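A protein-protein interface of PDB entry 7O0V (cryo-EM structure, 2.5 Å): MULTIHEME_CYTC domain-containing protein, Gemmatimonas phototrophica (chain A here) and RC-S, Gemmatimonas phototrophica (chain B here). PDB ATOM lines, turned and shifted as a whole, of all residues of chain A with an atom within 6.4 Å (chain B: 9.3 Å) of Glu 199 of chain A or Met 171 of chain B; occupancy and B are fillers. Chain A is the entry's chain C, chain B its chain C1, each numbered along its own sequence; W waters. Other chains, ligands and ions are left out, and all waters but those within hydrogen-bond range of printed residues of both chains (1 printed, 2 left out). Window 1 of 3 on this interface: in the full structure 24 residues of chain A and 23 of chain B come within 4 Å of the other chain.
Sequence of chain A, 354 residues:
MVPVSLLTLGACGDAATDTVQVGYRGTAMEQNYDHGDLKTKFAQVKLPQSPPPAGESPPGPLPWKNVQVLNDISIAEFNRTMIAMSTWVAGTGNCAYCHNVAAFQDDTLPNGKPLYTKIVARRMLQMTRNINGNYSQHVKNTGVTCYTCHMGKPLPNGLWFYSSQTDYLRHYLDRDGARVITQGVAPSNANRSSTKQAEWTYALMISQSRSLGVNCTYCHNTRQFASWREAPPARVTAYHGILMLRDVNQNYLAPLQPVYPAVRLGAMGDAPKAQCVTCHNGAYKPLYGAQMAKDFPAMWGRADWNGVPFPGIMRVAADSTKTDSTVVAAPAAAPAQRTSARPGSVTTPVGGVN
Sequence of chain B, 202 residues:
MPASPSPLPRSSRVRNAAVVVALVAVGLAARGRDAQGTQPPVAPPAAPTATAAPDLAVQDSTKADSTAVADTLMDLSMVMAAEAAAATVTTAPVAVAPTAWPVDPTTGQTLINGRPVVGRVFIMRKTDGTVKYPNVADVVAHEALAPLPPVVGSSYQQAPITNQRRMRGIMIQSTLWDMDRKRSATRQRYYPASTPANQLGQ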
ATOM      1  N   TYR A 168     -19.721  -3.795 -16.785  1.00  0.00           N
ATOM      2  CA  TYR A 168     -20.453  -2.546 -16.582  1.00  0.00           C
ATOM      3  C   TYR A 168     -21.887  -2.736 -16.094  1.00  0.00           C
ATOM      4  O   TYR A 168     -22.473  -1.780 -15.581  1.00  0.00           O
ATOM      5  CB  TYR A 168     -20.434  -1.696 -17.860  1.00  0.00           C
ATOM      6  CG  TYR A 168     -20.991  -2.350 -19.107  1.00  0.00           C
ATOM      7  CD1 TYR A 168     -22.344  -2.639 -19.235  1.00  0.00           C
ATOM      8  CD2 TYR A 168     -20.160  -2.641 -20.178  1.00  0.00           C
ATOM      9  CE1 TYR A 168     -22.838  -3.248 -20.369  1.00  0.00           C
ATOM     10  CE2 TYR A 168     -20.649  -3.228 -21.323  1.00  0.00           C
ATOM     11  CZ  TYR A 168     -21.986  -3.535 -21.412  1.00  0.00           C
ATOM     12  OH  TYR A 168     -22.475  -4.102 -22.564  1.00  0.00           O
ATOM     13  N   SER A 194      -9.500   8.509 -15.262  1.00  0.00           N
ATOM     14  CA  SER A 194      -8.685   7.995 -16.353  1.00  0.00           C
ATOM     15  C   SER A 194      -9.446   8.011 -17.681  1.00  0.00           C
ATOM     16  O   SER A 194     -10.679   7.987 -17.726  1.00  0.00           O
ATOM     17  CB  SER A 194      -8.219   6.575 -16.039  1.00  0.00           C
ATOM     18  OG  SER A 194      -7.508   6.017 -17.128  1.00  0.00           O
ATOM     19  N   THR A 195      -8.681   8.043 -18.776  1.00  0.00           N
ATOM     20  CA  THR A 195      -9.231   7.749 -20.099  1.00  0.00           C
ATOM     21  C   THR A 195      -9.827   6.346 -20.182  1.00  0.00           C
ATOM     22  O   THR A 195     -10.808   6.133 -20.901  1.00  0.00           O
ATOM     23  CB  THR A 195      -8.147   7.924 -21.167  1.00  0.00           C
ATOM     24  OG1 THR A 195      -7.524   9.202 -21.010  1.00  0.00           O
ATOM     25  CG2 THR A 195      -8.745   7.839 -22.562  1.00  0.00           C
ATOM     26  N   LYS A 196      -9.257   5.384 -19.450  1.00  0.00           N
ATOM     27  CA  LYS A 196      -9.871   4.063 -19.331  1.00  0.00           C
ATOM     28  C   LYS A 196     -11.255   4.120 -18.700  1.00  0.00           C
ATOM     29  O   LYS A 196     -12.150   3.361 -19.085  1.00  0.00           O
ATOM     30  CB  LYS A 196      -8.970   3.142 -18.515  1.00  0.00           C
ATOM     31  CG  LYS A 196      -7.616   2.900 -19.127  1.00  0.00           C
ATOM     32  CD  LYS A 196      -6.961   1.699 -18.486  1.00  0.00           C
ATOM     33  CE  LYS A 196      -5.549   1.519 -18.984  1.00  0.00           C
ATOM     34  NZ  LYS A 196      -5.224   0.082 -19.141  1.00  0.00           N
ATOM     35  N   GLN A 197     -11.451   5.007 -17.728  1.00  0.00           N
ATOM     36  CA  GLN A 197     -12.774   5.162 -17.135  1.00  0.00           C
ATOM     37  C   GLN A 197     -13.768   5.772 -18.118  1.00  0.00           C
ATOM     38  O   GLN A 197     -14.945   5.399 -18.125  1.00  0.00           O
ATOM     39  CB  GLN A 197     -12.672   5.986 -15.855  1.00  0.00           C
ATOM     40  CG  GLN A 197     -11.972   5.231 -14.736  1.00  0.00           C
ATOM     41  CD  GLN A 197     -11.837   6.039 -13.469  1.00  0.00           C
ATOM     42  OE1 GLN A 197     -11.302   7.142 -13.482  1.00  0.00           O
ATOM     43  NE2 GLN A 197     -12.318   5.491 -12.362  1.00  0.00           N
ATOM     44  N   ALA A 198     -13.316   6.711 -18.951  1.00  0.00           N
ATOM     45  CA  ALA A 198     -14.156   7.198 -20.041  1.00  0.00           C
ATOM     46  C   ALA A 198     -14.519   6.088 -21.027  1.00  0.00           C
ATOM     47  O   ALA A 198     -15.646   6.050 -21.532  1.00  0.00           O
ATOM     48  CB  ALA A 198     -13.457   8.348 -20.765  1.00  0.00           C
ATOM     49  N   GLU A 199     -13.584   5.180 -21.316  1.00  0.00           N
ATOM     50  CA  GLU A 199     -13.914   4.002 -22.117  1.00  0.00           C
ATOM     51  C   GLU A 199     -14.953   3.113 -21.443  1.00  0.00           C
ATOM     52  O   GLU A 199     -15.827   2.555 -22.116  1.00  0.00           O
ATOM     53  CB  GLU A 199     -12.656   3.186 -22.421  1.00  0.00           C
ATOM     54  CG  GLU A 199     -11.718   3.830 -23.411  1.00  0.00           C
ATOM     55  CD  GLU A 199     -10.410   3.088 -23.568  1.00  0.00           C
ATOM     56  OE1 GLU A 199      -9.508   3.285 -22.729  1.00  0.00           O
ATOM     57  OE2 GLU A 199     -10.279   2.318 -24.540  1.00  0.00           O
ATOM     58  N   TRP A 200     -14.875   2.963 -20.121  1.00  0.00           N
ATOM     59  CA  TRP A 200     -15.861   2.154 -19.410  1.00  0.00           C
ATOM     60  C   TRP A 200     -17.252   2.778 -19.449  1.00  0.00           C
ATOM     61  O   TRP A 200     -18.243   2.077 -19.675  1.00  0.00           O
ATOM     62  CB  TRP A 200     -15.407   1.946 -17.968  1.00  0.00           C
ATOM     63  CG  TRP A 200     -16.274   1.028 -17.169  1.00  0.00           C
ATOM     64  CD1 TRP A 200     -16.127  -0.320 -17.036  1.00  0.00           C
ATOM     65  CD2 TRP A 200     -17.412   1.387 -16.378  1.00  0.00           C
ATOM     66  NE1 TRP A 200     -17.106  -0.825 -16.218  1.00  0.00           N
ATOM     67  CE2 TRP A 200     -17.908   0.203 -15.800  1.00  0.00           C
ATOM     68  CE3 TRP A 200     -18.063   2.593 -16.106  1.00  0.00           C
ATOM     69  CZ2 TRP A 200     -19.022   0.190 -14.965  1.00  0.00           C
ATOM     70  CZ3 TRP A 200     -19.171   2.577 -15.279  1.00  0.00           C
ATOM     71  CH2 TRP A 200     -19.639   1.384 -14.719  1.00  0.00           C
ATOM     72  N   THR A 201     -17.348   4.090 -19.229  1.00  0.00           N
ATOM     73  CA  THR A 201     -18.630   4.775 -19.369  1.00  0.00           C
ATOM     74  C   THR A 201     -19.152   4.694 -20.799  1.00  0.00           C
ATOM     75  O   THR A 201     -20.355   4.514 -21.020  1.00  0.00           O
ATOM     76  CB  THR A 201     -18.496   6.232 -18.927  1.00  0.00           C
ATOM     77  OG1 THR A 201     -18.179   6.278 -17.532  1.00  0.00           O
ATOM     78  CG2 THR A 201     -19.791   6.991 -19.156  1.00  0.00           C
ATOM     79  N   TYR A 202     -18.259   4.804 -21.780  1.00  0.00           N
ATOM     80  CA  TYR A 202     -18.650   4.683 -23.181  1.00  0.00           C
ATOM     81  C   TYR A 202     -19.222   3.302 -23.491  1.00  0.00           C
ATOM     82  O   TYR A 202     -20.231   3.188 -24.195  1.00  0.00           O
ATOM     83  CB  TYR A 202     -17.428   4.992 -24.053  1.00  0.00           C
ATOM     84  CG  TYR A 202     -17.673   5.249 -25.525  1.00  0.00           C
ATOM     85  CD1 TYR A 202     -18.953   5.290 -26.056  1.00  0.00           C
ATOM     86  CD2 TYR A 202     -16.609   5.512 -26.375  1.00  0.00           C
ATOM     87  CE1 TYR A 202     -19.159   5.526 -27.401  1.00  0.00           C
ATOM     88  CE2 TYR A 202     -16.806   5.768 -27.716  1.00  0.00           C
ATOM     89  CZ  TYR A 202     -18.083   5.772 -28.224  1.00  0.00           C
ATOM     90  OH  TYR A 202     -18.285   6.039 -29.557  1.00  0.00           O
ATOM     91  N   ALA A 203     -18.597   2.243 -22.973  1.00  0.00           N
ATOM     92  CA  ALA A 203     -19.154   0.898 -23.107  1.00  0.00           C
ATOM     93  C   ALA A 203     -20.522   0.771 -22.442  1.00  0.00           C
ATOM     94  O   ALA A 203     -21.458   0.214 -23.025  1.00  0.00           O
ATOM     95  CB  ALA A 203     -18.181  -0.126 -22.524  1.00  0.00           C
ATOM     96  N   LEU A 204     -20.651   1.271 -21.210  1.00  0.00           N
ATOM     97  CA  LEU A 204     -21.949   1.324 -20.539  1.00  0.00           C
ATOM     98  C   LEU A 204     -23.005   2.051 -21.365  1.00  0.00           C
ATOM     99  O   LEU A 204     -24.154   1.603 -21.451  1.00  0.00           O
ATOM    100  CB  LEU A 204     -21.793   1.988 -19.171  1.00  0.00           C
ATOM    101  CG  LEU A 204     -23.069   2.294 -18.388  1.00  0.00           C
ATOM    102  CD1 LEU A 204     -23.747   1.012 -17.935  1.00  0.00           C
ATOM    103  CD2 LEU A 204     -22.754   3.183 -17.203  1.00  0.00           C
ATOM    104  N   ILE A 206     -23.137   2.676 -24.696  1.00  0.00           N
ATOM    105  CA  ILE A 206     -23.546   1.910 -25.870  1.00  0.00           C
ATOM    106  C   ILE A 206     -24.609   0.880 -25.503  1.00  0.00           C
ATOM    107  O   ILE A 206     -25.591   0.694 -26.230  1.00  0.00           O
ATOM    108  CB  ILE A 206     -22.317   1.253 -26.527  1.00  0.00           C
ATOM    109  CG1 ILE A 206     -21.446   2.312 -27.203  1.00  0.00           C
ATOM    110  CG2 ILE A 206     -22.740   0.210 -27.543  1.00  0.00           C
ATOM    111  CD1 ILE A 206     -20.101   1.798 -27.656  1.00  0.00           C
ATOM    112  N   ARG B 165     -10.600 -11.679 -16.869  1.00  0.00           N
ATOM    113  CA  ARG B 165     -10.636 -11.599 -18.325  1.00  0.00           C
ATOM    114  C   ARG B 165      -9.242 -11.759 -18.919  1.00  0.00           C
ATOM    115  O   ARG B 165      -8.271 -11.174 -18.434  1.00  0.00           O
ATOM    116  CB  ARG B 165     -11.215 -10.258 -18.772  1.00  0.00           C
ATOM    117  CG  ARG B 165     -12.686 -10.050 -18.500  1.00  0.00           C
ATOM    118  CD  ARG B 165     -13.102  -8.675 -18.996  1.00  0.00           C
ATOM    119  NE  ARG B 165     -14.506  -8.385 -18.737  1.00  0.00           N
ATOM    120  CZ  ARG B 165     -15.137  -7.304 -19.172  1.00  0.00           C
ATOM    121  NH1 ARG B 165     -14.507  -6.366 -19.861  1.00  0.00           N
ATOM    122  NH2 ARG B 165     -16.429  -7.152 -18.899  1.00  0.00           N
ATOM    123  N   MET B 167      -8.825 -10.633 -22.033  1.00  0.00           N
ATOM    124  CA  MET B 167      -8.747  -9.420 -22.840  1.00  0.00           C
ATOM    125  C   MET B 167      -8.902  -8.191 -21.954  1.00  0.00           C
ATOM    126  O   MET B 167      -9.956  -7.989 -21.342  1.00  0.00           O
ATOM    127  CB  MET B 167      -9.804  -9.449 -23.942  1.00  0.00           C
ATOM    128  CG  MET B 167      -9.453 -10.439 -25.040  1.00  0.00           C
ATOM    129  SD  MET B 167     -10.672 -10.559 -26.352  1.00  0.00           S
ATOM    130  CE  MET B 167     -10.300  -9.066 -27.258  1.00  0.00           C
ATOM    131  N   ARG B 168      -7.854  -7.374 -21.891  1.00  0.00           N
ATOM    132  CA  ARG B 168      -7.836  -6.194 -21.038  1.00  0.00           C
ATOM    133  C   ARG B 168      -8.447  -4.955 -21.685  1.00  0.00           C
ATOM    134  O   ARG B 168      -8.592  -3.936 -21.002  1.00  0.00           O
ATOM    135  CB  ARG B 168      -6.404  -5.906 -20.577  1.00  0.00           C
ATOM    136  CG  ARG B 168      -5.871  -6.996 -19.657  1.00  0.00           C
ATOM    137  CD  ARG B 168      -4.443  -6.756 -19.206  1.00  0.00           C
ATOM    138  NE  ARG B 168      -4.303  -5.493 -18.493  1.00  0.00           N
ATOM    139  CZ  ARG B 168      -3.622  -4.447 -18.940  1.00  0.00           C
ATOM    140  NH1 ARG B 168      -2.903  -4.514 -20.046  1.00  0.00           N
ATOM    141  NH2 ARG B 168      -3.632  -3.320 -18.236  1.00  0.00           N
ATOM    142  N   GLY B 169      -8.787  -5.000 -22.975  1.00  0.00           N
ATOM    143  CA  GLY B 169      -9.414  -3.864 -23.632  1.00  0.00           C
ATOM    144  C   GLY B 169     -10.722  -3.475 -22.970  1.00  0.00           C
ATOM    145  O   GLY B 169     -11.577  -4.329 -22.724  1.00  0.00           O
ATOM    146  N   ILE B 170     -10.887  -2.184 -22.668  1.00  0.00           N
ATOM    147  CA  ILE B 170     -11.956  -1.766 -21.764  1.00  0.00           C
ATOM    148  C   ILE B 170     -13.342  -1.852 -22.407  1.00  0.00           C
ATOM    149  O   ILE B 170     -14.323  -2.168 -21.724  1.00  0.00           O
ATOM    150  CB  ILE B 170     -11.662  -0.342 -21.250  1.00  0.00           C
ATOM    151  CG1 ILE B 170     -10.355  -0.316 -20.452  1.00  0.00           C
ATOM    152  CG2 ILE B 170     -12.797   0.170 -20.380  1.00  0.00           C
ATOM    153  CD1 ILE B 170     -10.343  -1.244 -19.261  1.00  0.00           C
ATOM    154  N   MET B 171     -13.458  -1.603 -23.710  1.00  0.00           N
ATOM    155  CA  MET B 171     -14.762  -1.565 -24.366  1.00  0.00           C
ATOM    156  C   MET B 171     -15.196  -2.891 -24.986  1.00  0.00           C
ATOM    157  O   MET B 171     -16.257  -2.938 -25.615  1.00  0.00           O
ATOM    158  CB  MET B 171     -14.782  -0.468 -25.436  1.00  0.00           C
ATOM    159  CG  MET B 171     -14.577   0.930 -24.872  1.00  0.00           C
ATOM    160  SD  MET B 171     -14.888   2.251 -26.057  1.00  0.00           S
ATOM    161  CE  MET B 171     -16.610   1.961 -26.441  1.00  0.00           C
ATOM    162  N   ILE B 172     -14.401  -3.951 -24.838  1.00  0.00           N
ATOM    163  CA  ILE B 172     -14.620  -5.196 -25.577  1.00  0.00           C
ATOM    164  C   ILE B 172     -16.017  -5.774 -25.338  1.00  0.00           C
ATOM    165  O   ILE B 172     -16.627  -6.345 -26.249  1.00  0.00           O
ATOM    166  CB  ILE B 172     -13.512  -6.212 -25.235  1.00  0.00           C
ATOM    167  CG1 ILE B 172     -13.527  -7.369 -26.233  1.00  0.00           C
ATOM    168  CG2 ILE B 172     -13.627  -6.705 -23.799  1.00  0.00           C
ATOM    169  CD1 ILE B 172     -13.097  -6.965 -27.618  1.00  0.00           C
ATOM    170  N   GLN B 173     -16.548  -5.632 -24.121  1.00  0.00           N
ATOM    171  CA  GLN B 173     -17.880  -6.150 -23.811  1.00  0.00           C
ATOM    172  C   GLN B 173     -18.986  -5.508 -24.648  1.00  0.00           C
ATOM    173  O   GLN B 173     -19.974  -6.176 -24.974  1.00  0.00           O
ATOM    174  CB  GLN B 173     -18.167  -5.980 -22.317  1.00  0.00           C
ATOM    175  CG  GLN B 173     -19.474  -6.600 -21.848  1.00  0.00           C
ATOM    176  CD  GLN B 173     -19.731  -6.375 -20.371  1.00  0.00           C
ATOM    177  OE1 GLN B 173     -18.837  -5.971 -19.630  1.00  0.00           O
ATOM    178  NE2 GLN B 173     -20.956  -6.641 -19.935  1.00  0.00           N
ATOM    179  N   SER B 174     -18.845  -4.236 -25.021  1.00  0.00           N
ATOM    180  CA  SER B 174     -19.814  -3.614 -25.920  1.00  0.00           C
ATOM    181  C   SER B 174     -19.459  -3.750 -27.395  1.00  0.00           C
ATOM    182  O   SER B 174     -20.346  -3.992 -28.219  1.00  0.00           O
ATOM    183  CB  SER B 174     -19.976  -2.132 -25.579  1.00  0.00           C
ATOM    184  OG  SER B 174     -20.586  -1.967 -24.314  1.00  0.00           O
ATOM    185  N   THR B 175     -18.188  -3.589 -27.755  1.00  0.00           N
ATOM    186  CA  THR B 175     -17.831  -3.537 -29.167  1.00  0.00           C
ATOM    187  C   THR B 175     -17.804  -4.917 -29.816  1.00  0.00           C
ATOM    188  O   THR B 175     -18.071  -5.030 -31.017  1.00  0.00           O
ATOM    189  CB  THR B 175     -16.480  -2.840 -29.350  1.00  0.00           C
ATOM    190  OG1 THR B 175     -15.483  -3.497 -28.559  1.00  0.00           O
ATOM    191  CG2 THR B 175     -16.575  -1.380 -28.935  1.00  0.00           C
ATOM    192  N   LEU B 176     -17.495  -5.968 -29.060  1.00  0.00           N
ATOM    193  CA  LEU B 176     -17.440  -7.315 -29.617  1.00  0.00           C
ATOM    194  C   LEU B 176     -18.423  -8.282 -28.974  1.00  0.00           C
ATOM    195  O   LEU B 176     -19.186  -8.940 -29.689  1.00  0.00           O
ATOM    196  CB  LEU B 176     -16.011  -7.870 -29.501  1.00  0.00           C
ATOM    197  CG  LEU B 176     -15.780  -9.271 -30.064  1.00  0.00           C
ATOM    198  CD1 LEU B 176     -16.056  -9.289 -31.549  1.00  0.00           C
ATOM    199  CD2 LEU B 176     -14.361  -9.728 -29.789  1.00  0.00           C
ATOM    200  N   TRP B 177     -18.426  -8.401 -27.646  1.00  0.00           N
ATOM    201  CA  TRP B 177     -19.130  -9.508 -27.004  1.00  0.00           C
ATOM    202  C   TRP B 177     -20.649  -9.366 -27.020  1.00  0.00           C
ATOM    203  O   TRP B 177     -21.343 -10.367 -26.810  1.00  0.00           O
ATOM    204  CB  TRP B 177     -18.657  -9.704 -25.561  1.00  0.00           C
ATOM    205  CG  TRP B 177     -17.194  -9.992 -25.410  1.00  0.00           C
ATOM    206  CD1 TRP B 177     -16.317 -10.324 -26.398  1.00  0.00           C
ATOM    207  CD2 TRP B 177     -16.457 -10.061 -24.183  1.00  0.00           C
ATOM    208  NE1 TRP B 177     -15.069 -10.550 -25.870  1.00  0.00           N
ATOM    209  CE2 TRP B 177     -15.130 -10.399 -24.510  1.00  0.00           C
ATOM    210  CE3 TRP B 177     -16.788  -9.854 -22.840  1.00  0.00           C
ATOM    211  CZ2 TRP B 177     -14.134 -10.534 -23.546  1.00  0.00           C
ATOM    212  CZ3 TRP B 177     -15.797  -9.987 -21.884  1.00  0.00           C
ATOM    213  CH2 TRP B 177     -14.487 -10.323 -22.242  1.00  0.00           C
ATOM    214  N   ASP B 178     -21.191  -8.168 -27.257  1.00  0.00           N
ATOM    215  CA  ASP B 178     -22.634  -8.059 -27.461  1.00  0.00           C
ATOM    216  C   ASP B 178     -23.089  -8.829 -28.695  1.00  0.00           C
ATOM    217  O   ASP B 178     -24.148  -9.466 -28.682  1.00  0.00           O
ATOM    218  CB  ASP B 178     -23.044  -6.591 -27.590  1.00  0.00           C
ATOM    219  CG  ASP B 178     -23.434  -5.964 -26.266  1.00  0.00           C
ATOM    220  OD1 ASP B 178     -23.539  -6.695 -25.260  1.00  0.00           O
ATOM    221  OD2 ASP B 178     -23.652  -4.733 -26.238  1.00  0.00           O
HETATM  222  O   HOH W   1     -24.283  -5.798 -22.710  1.00  0.00           O
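Among the printed residues, merely in contact across the chains: Tyr 168 of chain A with Gln 173 of chain B (3.4 Å), Glu 199 of chain A with Met 171 of chain B (3.4 Å), Trp 200 of chain A with Ile 170 of chain B (3.5 Å), Lys 196 of chain A with Ile 170 of chain B (3.5 Å), Tyr 202 of chain A with Met 171 of chain B (3.6 Å), Glu 199 of chain A with Ile 170 of chain B (3.6 Å), Ile 206 of chain A with Met 171 of chain B (3.7 Å), Lys 196 of chain A with Arg 168 of chain B (3.9 Å) and Tyr 168 of chain A with Asp 178 of chain B (3.9 Å).
The side-chain hydroxyl of Tyr 168 of chain A sits close to the side-chain hydroxyl of Ser 174 of chain B (3.3 Å). O of Ala 203 of chain A lies within hydrogen-bond range of OG of Ser 174 of chain B (2.7 Å).
Of the printed residues of chain B, Lys 196 of chain A touches Arg 168 (3.9 Å) and Ile 170 (3.5 Å). No residue of chain B comes within 4 Å of Ala 198 of chain A. Of chain B, only Ile 170 and Met 171 come within 4 Å of Glu 199 of chain A. Printed residues of chain A within 4 Å of Ile 170 of chain B: Lys 196 (3.5 Å), Glu 199 (3.6 Å) and Trp 200 (3.5 Å). Of the printed residues of chain A, Met 171 of chain B touches Glu 199, Tyr 202 and Ile 206. Printed residues of chain A within 4 Å of Gln 173 of chain B: Tyr 168 (3.4 Å). Of the printed residues of chain A, Asp 178 of chain B touches Tyr 168 (3.9 Å). The nearest residue of chain B that does not touch Glu 199 of chain A is Gly 169 of chain B (6.0 Å).
The side-chain hydroxyl (OG) of Ser 194 of chain A is in hydrogen-bond range of the backbone NH (N) of Lys 196 of chain A (3.0 Å). The side-chain amide oxygen (OE1) of Gln 173 of chain B is in hydrogen-bond range of the guanidinium group (NH2) of Arg 165 of chain B, 2.8 Å away. O of Met 171 of chain B sits at hydrogen-bond distance from OG1 of Thr 175 of chain B, at 3.1 Å. The backbone carbonyl oxygen (O) of Gln 173 of chain B lies within hydrogen-bond range of the backbone NH (N) of Asp 178 of chain B.
Hydrophobic or aromatic side chains of chain A within 4 Å of the printed part of chain B: Tyr 168, Trp 200, Tyr 202, Ala 203 and Ile 206.
Water W1 bridges the side-chain hydroxyl (OH) of Tyr 168 of chain A (2.5 Å) and the side-chain carboxylate (OD1) of Asp 178 of chain B (2.8 Å).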
